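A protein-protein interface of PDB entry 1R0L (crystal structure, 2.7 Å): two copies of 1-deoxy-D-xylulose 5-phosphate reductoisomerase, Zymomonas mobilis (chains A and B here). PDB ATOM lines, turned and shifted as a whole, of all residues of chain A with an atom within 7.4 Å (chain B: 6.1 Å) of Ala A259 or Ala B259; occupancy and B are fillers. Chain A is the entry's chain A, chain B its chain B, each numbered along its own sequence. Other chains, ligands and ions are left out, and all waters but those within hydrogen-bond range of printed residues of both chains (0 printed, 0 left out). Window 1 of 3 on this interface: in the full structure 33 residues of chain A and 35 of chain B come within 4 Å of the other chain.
The side-chain amide oxygen of Gln B260 is in hydrogen-bond range of the side-chain hydroxyl of Ser A256 (2.9 Å).
N of Ile B261 sits at hydrogen-bond distance from O of Ile A257 (2.7 Å).
O of Ala A259 lies within hydrogen-bond range of N of Ala B259.
The backbone carbonyl oxygen of Ile B257 sits at hydrogen-bond distance from the backbone NH of Ile A261, 2.7 Å away.
The side-chain sulfur of Cys A159 lies within hydrogen-bond range of the backbone carbonyl oxygen of Leu A258, at 3.5 Å.
SG of Cys A159 lies within hydrogen-bond range of N of Gln A260 (3.5 Å).
O of Val A250 is in hydrogen-bond range of N of Leu A258 (3.0 Å).
SG of Cys B159 sits at hydrogen-bond distance from O of Leu B258 (3.5 Å).
SG of Cys B159 lies close to N of Ala B259 (3.6 Å).
SG of Cys B159 is in hydrogen-bond range of N of Gln B260.
Gln A158 touches Leu B258.
O of Ala B259 touches O of Ile A257, 3.6 Å away.
Ile A257 touches Gln B260.
Leu A258 touches Ala B259 (CA to O, 3.4 Å).
O of Ala A259 touches O of Ile B257 (3.6 Å).
Ala A259 touches Leu B258 (O to CA, 3.4 Å).
Ala A259 touches Ile B261.
Gln A260 touches Ile B257.
Phe A289 touches Met B249.
CE1 of Phe A289 touches CD1 of Ile B257, at 3.9 Å.
Ala A155 touches none of the printed residues of chain B.
Of chain B, only Ile B257 (3.6 Å), Leu B258 (3.4 Å), Ala B259 (2.9 Å) and Ile B261 (3.9 Å) come within 4 Å of Ala A259.
Printed residues of chain B within 4 Å of Gln A260: Ile B257 (3.4 Å).
Cys B159 touches none of the printed residues of chain A.
Of the printed residues of chain A, Met B249 touches Phe A289.
Of the printed residues of chain A, Ile B257 touches Ala A259, Gln A260, Ile A261 and Phe A289.
Of chain A, only Ile A257, Leu A258 and Ala A259 come within 4 Å of Ala B259.
Of the printed residues of chain A, Gln B260 touches Ser A256 (2.9 Å) and Ile A257 (3.4 Å).
Printed residues of chain A within 4 Å of Ile B261: Ser A256 (3.97 Å), Ile A257 (2.7 Å) and Ala A259 (3.9 Å).
The nearest residue of chain B that does not touch Ala A259 is Gln B260 (5.1 Å).
The nearest printed residue of chain B that does not touch Phe A289 is Ile B246 (5.1 Å).
Hydrophobic or aromatic side chains of chain A that line the printed part of chain B: Ile A257, Leu A258, Ala A259 and Phe A289.
Of the 11 printed residues of chain B, 6 touch a printed residue of chain A.
Among the printed residues, 15 pairs touch across the chains.
Among the printed residues, no Asp or Glu carboxylate lies within 4 Å of a Lys or Arg side-chain nitrogen of the other chain.
Ile A257 touches Ile B261, and with the chains exchanged Ile A261 touches Ile B257.
Leu A258 touches Ala B259, and with the chains exchanged Ala A259 touches Leu B258.
Ala A259 touches its own counterpart, Ala B259.
Ala A259 touches Ile B261, but with the chains exchanged Ile A261 does not touch Ala B259 (4.1 Å).
Positions printed for both chains: 155, 159, 246, 248, 249, 250, 257, 258, 259, 260 and 261.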
ATOM      1  N   ALA A 155      -3.634  22.907  16.907  1.00  0.00           N
ATOM      2  CA  ALA A 155      -5.016  22.647  17.293  1.00  0.00           C
ATOM      3  C   ALA A 155      -5.789  22.252  16.022  1.00  0.00           C
ATOM      4  O   ALA A 155      -6.445  21.216  15.985  1.00  0.00           O
ATOM      5  CB  ALA A 155      -5.623  23.893  17.929  1.00  0.00           C
ATOM      6  N   ILE A 156      -5.688  23.076  14.979  1.00  0.00           N
ATOM      7  CA  ILE A 156      -6.346  22.812  13.690  1.00  0.00           C
ATOM      8  C   ILE A 156      -5.954  21.428  13.139  1.00  0.00           C
ATOM      9  O   ILE A 156      -6.798  20.640  12.687  1.00  0.00           O
ATOM     10  CB  ILE A 156      -5.936  23.873  12.630  1.00  0.00           C
ATOM     11  CG1 ILE A 156      -6.553  25.240  12.964  1.00  0.00           C
ATOM     12  CG2 ILE A 156      -6.339  23.401  11.228  1.00  0.00           C
ATOM     13  CD1 ILE A 156      -5.831  26.421  12.254  1.00  0.00           C
ATOM     14  N   GLN A 158      -5.043  18.797  14.698  1.00  0.00           N
ATOM     15  CA  GLN A 158      -5.672  17.686  15.425  1.00  0.00           C
ATOM     16  C   GLN A 158      -7.161  17.520  15.151  1.00  0.00           C
ATOM     17  O   GLN A 158      -7.742  16.479  15.479  1.00  0.00           O
ATOM     18  CB  GLN A 158      -5.465  17.806  16.934  1.00  0.00           C
ATOM     19  CG  GLN A 158      -4.062  17.479  17.415  1.00  0.00           C
ATOM     20  CD  GLN A 158      -3.948  17.617  18.917  1.00  0.00           C
ATOM     21  OE1 GLN A 158      -4.641  16.933  19.655  1.00  0.00           O
ATOM     22  NE2 GLN A 158      -3.085  18.512  19.373  1.00  0.00           N
ATOM     23  N   CYS A 159      -7.774  18.542  14.554  1.00  0.00           N
ATOM     24  CA  CYS A 159      -9.198  18.518  14.229  1.00  0.00           C
ATOM     25  C   CYS A 159      -9.382  18.461  12.717  1.00  0.00           C
ATOM     26  O   CYS A 159     -10.518  18.442  12.211  1.00  0.00           O
ATOM     27  CB  CYS A 159      -9.865  19.791  14.733  1.00  0.00           C
ATOM     28  SG  CYS A 159      -9.538  20.172  16.428  1.00  0.00           S
ATOM     29  N   ILE A 246      -9.880  27.573  23.838  1.00  0.00           N
ATOM     30  CA  ILE A 246     -10.145  26.849  22.597  1.00  0.00           C
ATOM     31  C   ILE A 246      -9.042  27.408  21.686  1.00  0.00           C
ATOM     32  O   ILE A 246      -9.007  28.618  21.408  1.00  0.00           O
ATOM     33  CB  ILE A 246     -11.506  27.198  21.992  1.00  0.00           C
ATOM     34  CG1 ILE A 246     -12.637  26.678  22.871  1.00  0.00           C
ATOM     35  CG2 ILE A 246     -11.633  26.571  20.625  1.00  0.00           C
ATOM     36  CD1 ILE A 246     -14.015  26.976  22.293  1.00  0.00           C
ATOM     37  N   HIS A 247      -8.142  26.533  21.232  1.00  0.00           N
ATOM     38  CA  HIS A 247      -7.001  26.931  20.415  1.00  0.00           C
ATOM     39  C   HIS A 247      -7.205  27.077  18.905  1.00  0.00           C
ATOM     40  O   HIS A 247      -6.299  27.558  18.198  1.00  0.00           O
ATOM     41  CB  HIS A 247      -5.842  25.967  20.678  1.00  0.00           C
ATOM     42  CG  HIS A 247      -5.434  25.882  22.121  1.00  0.00           C
ATOM     43  ND1 HIS A 247      -5.424  26.970  22.961  1.00  0.00           N
ATOM     44  CD2 HIS A 247      -4.990  24.844  22.863  1.00  0.00           C
ATOM     45  CE1 HIS A 247      -4.996  26.608  24.155  1.00  0.00           C
ATOM     46  NE2 HIS A 247      -4.726  25.321  24.121  1.00  0.00           N
ATOM     47  N   SER A 248      -8.384  26.662  18.430  1.00  0.00           N
ATOM     48  CA  SER A 248      -8.778  26.726  17.019  1.00  0.00           C
ATOM     49  C   SER A 248      -9.793  25.633  16.718  1.00  0.00           C
ATOM     50  O   SER A 248      -9.904  24.669  17.467  1.00  0.00           O
ATOM     51  CB  SER A 248      -7.576  26.602  16.090  1.00  0.00           C
ATOM     52  OG  SER A 248      -7.149  27.893  15.672  1.00  0.00           O
ATOM     53  N   MET A 249     -10.537  25.780  15.622  1.00  0.00           N
ATOM     54  CA  MET A 249     -11.580  24.813  15.287  1.00  0.00           C
ATOM     55  C   MET A 249     -11.681  24.511  13.795  1.00  0.00           C
ATOM     56  O   MET A 249     -11.177  25.257  12.966  1.00  0.00           O
ATOM     57  CB  MET A 249     -12.933  25.338  15.777  1.00  0.00           C
ATOM     58  CG  MET A 249     -12.915  25.875  17.198  1.00  0.00           C
ATOM     59  SD  MET A 249     -14.498  26.561  17.689  1.00  0.00           S
ATOM     60  CE  MET A 249     -14.209  28.263  17.385  1.00  0.00           C
ATOM     61  N   VAL A 250     -12.368  23.420  13.472  1.00  0.00           N
ATOM     62  CA  VAL A 250     -12.547  22.968  12.100  1.00  0.00           C
ATOM     63  C   VAL A 250     -13.968  22.434  11.924  1.00  0.00           C
ATOM     64  O   VAL A 250     -14.321  21.423  12.530  1.00  0.00           O
ATOM     65  CB  VAL A 250     -11.571  21.810  11.768  1.00  0.00           C
ATOM     66  CG1 VAL A 250     -11.836  21.296  10.369  1.00  0.00           C
ATOM     67  CG2 VAL A 250     -10.130  22.267  11.923  1.00  0.00           C
ATOM     68  N   SER A 256     -20.773  19.270  11.944  1.00  0.00           N
ATOM     69  CA  SER A 256     -19.963  18.902  13.095  1.00  0.00           C
ATOM     70  C   SER A 256     -18.660  19.696  13.209  1.00  0.00           C
ATOM     71  O   SER A 256     -17.854  19.723  12.280  1.00  0.00           O
ATOM     72  CB  SER A 256     -19.662  17.403  13.039  1.00  0.00           C
ATOM     73  OG  SER A 256     -18.718  17.046  14.023  1.00  0.00           O
ATOM     74  N   ILE A 257     -18.458  20.345  14.355  1.00  0.00           N
ATOM     75  CA  ILE A 257     -17.236  21.121  14.584  1.00  0.00           C
ATOM     76  C   ILE A 257     -16.299  20.475  15.619  1.00  0.00           C
ATOM     77  O   ILE A 257     -16.686  20.206  16.750  1.00  0.00           O
ATOM     78  CB  ILE A 257     -17.560  22.534  15.053  1.00  0.00           C
ATOM     79  CG1 ILE A 257     -18.497  23.222  14.049  1.00  0.00           C
ATOM     80  CG2 ILE A 257     -16.276  23.295  15.227  1.00  0.00           C
ATOM     81  CD1 ILE A 257     -18.954  24.632  14.489  1.00  0.00           C
ATOM     82  N   LEU A 258     -15.066  20.199  15.221  1.00  0.00           N
ATOM     83  CA  LEU A 258     -14.088  19.620  16.138  1.00  0.00           C
ATOM     84  C   LEU A 258     -13.190  20.749  16.646  1.00  0.00           C
ATOM     85  O   LEU A 258     -12.718  21.555  15.859  1.00  0.00           O
ATOM     86  CB  LEU A 258     -13.248  18.566  15.422  1.00  0.00           C
ATOM     87  CG  LEU A 258     -14.023  17.332  14.934  1.00  0.00           C
ATOM     88  CD1 LEU A 258     -13.080  16.348  14.289  1.00  0.00           C
ATOM     89  CD2 LEU A 258     -14.732  16.680  16.101  1.00  0.00           C
ATOM     90  N   ALA A 259     -12.977  20.833  17.956  1.00  0.00           N
ATOM     91  CA  ALA A 259     -12.120  21.878  18.509  1.00  0.00           C
ATOM     92  C   ALA A 259     -11.074  21.291  19.420  1.00  0.00           C
ATOM     93  O   ALA A 259     -11.309  20.283  20.085  1.00  0.00           O
ATOM     94  CB  ALA A 259     -12.943  22.898  19.285  1.00  0.00           C
ATOM     95  N   GLN A 260      -9.912  21.928  19.447  1.00  0.00           N
ATOM     96  CA  GLN A 260      -8.829  21.492  20.311  1.00  0.00           C
ATOM     97  C   GLN A 260      -8.773  22.509  21.461  1.00  0.00           C
ATOM     98  O   GLN A 260      -8.623  23.710  21.237  1.00  0.00           O
ATOM     99  CB  GLN A 260      -7.512  21.455  19.529  1.00  0.00           C
ATOM    100  CG  GLN A 260      -6.429  20.592  20.163  1.00  0.00           C
ATOM    101  CD  GLN A 260      -5.712  21.306  21.283  1.00  0.00           C
ATOM    102  OE1 GLN A 260      -4.954  20.696  22.050  1.00  0.00           O
ATOM    103  NE2 GLN A 260      -5.932  22.615  21.376  1.00  0.00           N
ATOM    104  N   ILE A 261      -8.932  22.016  22.687  1.00  0.00           N
ATOM    105  CA  ILE A 261      -8.921  22.861  23.871  1.00  0.00           C
ATOM    106  C   ILE A 261      -7.883  22.334  24.859  1.00  0.00           C
ATOM    107  O   ILE A 261      -7.469  21.171  24.784  1.00  0.00           O
ATOM    108  CB  ILE A 261     -10.309  22.861  24.550  1.00  0.00           C
ATOM    109  CG1 ILE A 261     -11.394  23.147  23.507  1.00  0.00           C
ATOM    110  CG2 ILE A 261     -10.363  23.910  25.625  1.00  0.00           C
ATOM    111  CD1 ILE A 261     -12.821  23.024  24.001  1.00  0.00           C
ATOM    112  N   PHE A 289     -12.425  22.900  33.716  1.00  0.00           N
ATOM    113  CA  PHE A 289     -13.488  23.766  33.249  1.00  0.00           C
ATOM    114  C   PHE A 289     -14.303  24.393  34.366  1.00  0.00           C
ATOM    115  O   PHE A 289     -14.956  25.421  34.153  1.00  0.00           O
ATOM    116  CB  PHE A 289     -14.402  23.022  32.302  1.00  0.00           C
ATOM    117  CG  PHE A 289     -13.733  22.594  31.036  1.00  0.00           C
ATOM    118  CD1 PHE A 289     -12.898  21.480  31.018  1.00  0.00           C
ATOM    119  CD2 PHE A 289     -13.978  23.273  29.838  1.00  0.00           C
ATOM    120  CE1 PHE A 289     -12.322  21.041  29.828  1.00  0.00           C
ATOM    121  CE2 PHE A 289     -13.405  22.841  28.638  1.00  0.00           C
ATOM    122  CZ  PHE A 289     -12.579  21.725  28.631  1.00  0.00           C
ATOM    123  N   ALA B 155     -20.417  12.544  19.986  1.00  0.00           N
ATOM    124  CA  ALA B 155     -19.415  13.588  20.129  1.00  0.00           C
ATOM    125  C   ALA B 155     -18.133  12.938  20.604  1.00  0.00           C
ATOM    126  O   ALA B 155     -17.056  13.191  20.045  1.00  0.00           O
ATOM    127  CB  ALA B 155     -19.863  14.597  21.120  1.00  0.00           C
ATOM    128  N   CYS B 159     -14.161  12.266  18.816  1.00  0.00           N
ATOM    129  CA  CYS B 159     -12.965  12.761  19.494  1.00  0.00           C
ATOM    130  C   CYS B 159     -12.154  11.616  20.130  1.00  0.00           C
ATOM    131  O   CYS B 159     -11.123  11.842  20.755  1.00  0.00           O
ATOM    132  CB  CYS B 159     -13.380  13.723  20.612  1.00  0.00           C
ATOM    133  SG  CYS B 159     -14.344  15.190  20.116  1.00  0.00           S
ATOM    134  N   ILE B 246     -21.078  22.338  23.475  1.00  0.00           N
ATOM    135  CA  ILE B 246     -20.013  21.339  23.426  1.00  0.00           C
ATOM    136  C   ILE B 246     -20.760  20.067  23.805  1.00  0.00           C
ATOM    137  O   ILE B 246     -21.342  19.997  24.895  1.00  0.00           O
ATOM    138  CB  ILE B 246     -18.941  21.591  24.484  1.00  0.00           C
ATOM    139  CG1 ILE B 246     -18.150  22.846  24.120  1.00  0.00           C
ATOM    140  CG2 ILE B 246     -18.063  20.342  24.641  1.00  0.00           C
ATOM    141  CD1 ILE B 246     -17.152  23.273  25.183  1.00  0.00           C
ATOM    142  N   SER B 248     -19.490  16.932  24.258  1.00  0.00           N
ATOM    143  CA  SER B 248     -18.645  16.013  25.035  1.00  0.00           C
ATOM    144  C   SER B 248     -17.197  16.186  24.593  1.00  0.00           C
ATOM    145  O   SER B 248     -16.936  16.708  23.523  1.00  0.00           O
ATOM    146  CB  SER B 248     -19.061  14.541  24.856  1.00  0.00           C
ATOM    147  OG  SER B 248     -19.786  14.074  25.987  1.00  0.00           O
ATOM    148  N   MET B 249     -16.265  15.734  25.414  1.00  0.00           N
ATOM    149  CA  MET B 249     -14.846  15.876  25.116  1.00  0.00           C
ATOM    150  C   MET B 249     -14.044  14.647  25.525  1.00  0.00           C
ATOM    151  O   MET B 249     -14.525  13.791  26.287  1.00  0.00           O
ATOM    152  CB  MET B 249     -14.288  17.078  25.864  1.00  0.00           C
ATOM    153  CG  MET B 249     -15.199  18.283  25.847  1.00  0.00           C
ATOM    154  SD  MET B 249     -14.496  19.644  26.811  1.00  0.00           S
ATOM    155  CE  MET B 249     -15.791  19.937  27.992  1.00  0.00           C
ATOM    156  N   VAL B 250     -12.814  14.576  25.015  1.00  0.00           N
ATOM    157  CA  VAL B 250     -11.894  13.479  25.310  1.00  0.00           C
ATOM    158  C   VAL B 250     -10.514  14.099  25.447  1.00  0.00           C
ATOM    159  O   VAL B 250     -10.017  14.713  24.504  1.00  0.00           O
ATOM    160  CB  VAL B 250     -11.846  12.449  24.160  1.00  0.00           C
ATOM    161  CG1 VAL B 250     -10.796  11.389  24.457  1.00  0.00           C
ATOM    162  CG2 VAL B 250     -13.213  11.815  23.962  1.00  0.00           C
ATOM    163  N   ILE B 257      -7.051  18.279  24.467  1.00  0.00           N
ATOM    164  CA  ILE B 257      -8.467  17.926  24.637  1.00  0.00           C
ATOM    165  C   ILE B 257      -9.238  18.168  23.342  1.00  0.00           C
ATOM    166  O   ILE B 257      -9.259  19.296  22.837  1.00  0.00           O
ATOM    167  CB  ILE B 257      -9.152  18.775  25.748  1.00  0.00           C
ATOM    168  CG1 ILE B 257      -8.552  18.446  27.114  1.00  0.00           C
ATOM    169  CG2 ILE B 257     -10.655  18.477  25.796  1.00  0.00           C
ATOM    170  CD1 ILE B 257      -9.300  19.075  28.280  1.00  0.00           C
ATOM    171  N   LEU B 258      -9.862  17.125  22.799  1.00  0.00           N
ATOM    172  CA  LEU B 258     -10.660  17.277  21.572  1.00  0.00           C
ATOM    173  C   LEU B 258     -12.126  17.327  21.989  1.00  0.00           C
ATOM    174  O   LEU B 258     -12.556  16.553  22.840  1.00  0.00           O
ATOM    175  CB  LEU B 258     -10.432  16.100  20.592  1.00  0.00           C
ATOM    176  CG  LEU B 258      -9.005  15.900  20.059  1.00  0.00           C
ATOM    177  CD1 LEU B 258      -8.925  14.719  19.123  1.00  0.00           C
ATOM    178  CD2 LEU B 258      -8.579  17.156  19.338  1.00  0.00           C
ATOM    179  N   ALA B 259     -12.883  18.254  21.409  1.00  0.00           N
ATOM    180  CA  ALA B 259     -14.314  18.392  21.705  1.00  0.00           C
ATOM    181  C   ALA B 259     -15.123  18.466  20.421  1.00  0.00           C
ATOM    182  O   ALA B 259     -14.652  18.946  19.396  1.00  0.00           O
ATOM    183  CB  ALA B 259     -14.576  19.635  22.536  1.00  0.00           C
ATOM    184  N   GLN B 260     -16.348  17.982  20.481  1.00  0.00           N
ATOM    185  CA  GLN B 260     -17.219  18.010  19.323  1.00  0.00           C
ATOM    186  C   GLN B 260     -18.263  19.059  19.660  1.00  0.00           C
ATOM    187  O   GLN B 260     -18.917  18.971  20.684  1.00  0.00           O
ATOM    188  CB  GLN B 260     -17.853  16.634  19.121  1.00  0.00           C
ATOM    189  CG  GLN B 260     -18.472  16.429  17.757  1.00  0.00           C
ATOM    190  CD  GLN B 260     -19.803  17.123  17.614  1.00  0.00           C
ATOM    191  OE1 GLN B 260     -20.286  17.332  16.494  1.00  0.00           O
ATOM    192  NE2 GLN B 260     -20.423  17.466  18.745  1.00  0.00           N
ATOM    193  N   ILE B 261     -18.396  20.068  18.821  1.00  0.00           N
ATOM    194  CA  ILE B 261     -19.341  21.145  19.062  1.00  0.00           C
ATOM    195  C   ILE B 261     -20.269  21.304  17.865  1.00  0.00           C
ATOM    196  O   ILE B 261     -20.004  20.778  16.784  1.00  0.00           O
ATOM    197  CB  ILE B 261     -18.584  22.466  19.304  1.00  0.00           C
ATOM    198  CG1 ILE B 261     -17.509  22.249  20.378  1.00  0.00           C
ATOM    199  CG2 ILE B 261     -19.541  23.553  19.749  1.00  0.00           C
ATOM    200  CD1 ILE B 261     -16.591  23.442  20.590  1.00  0.00           C
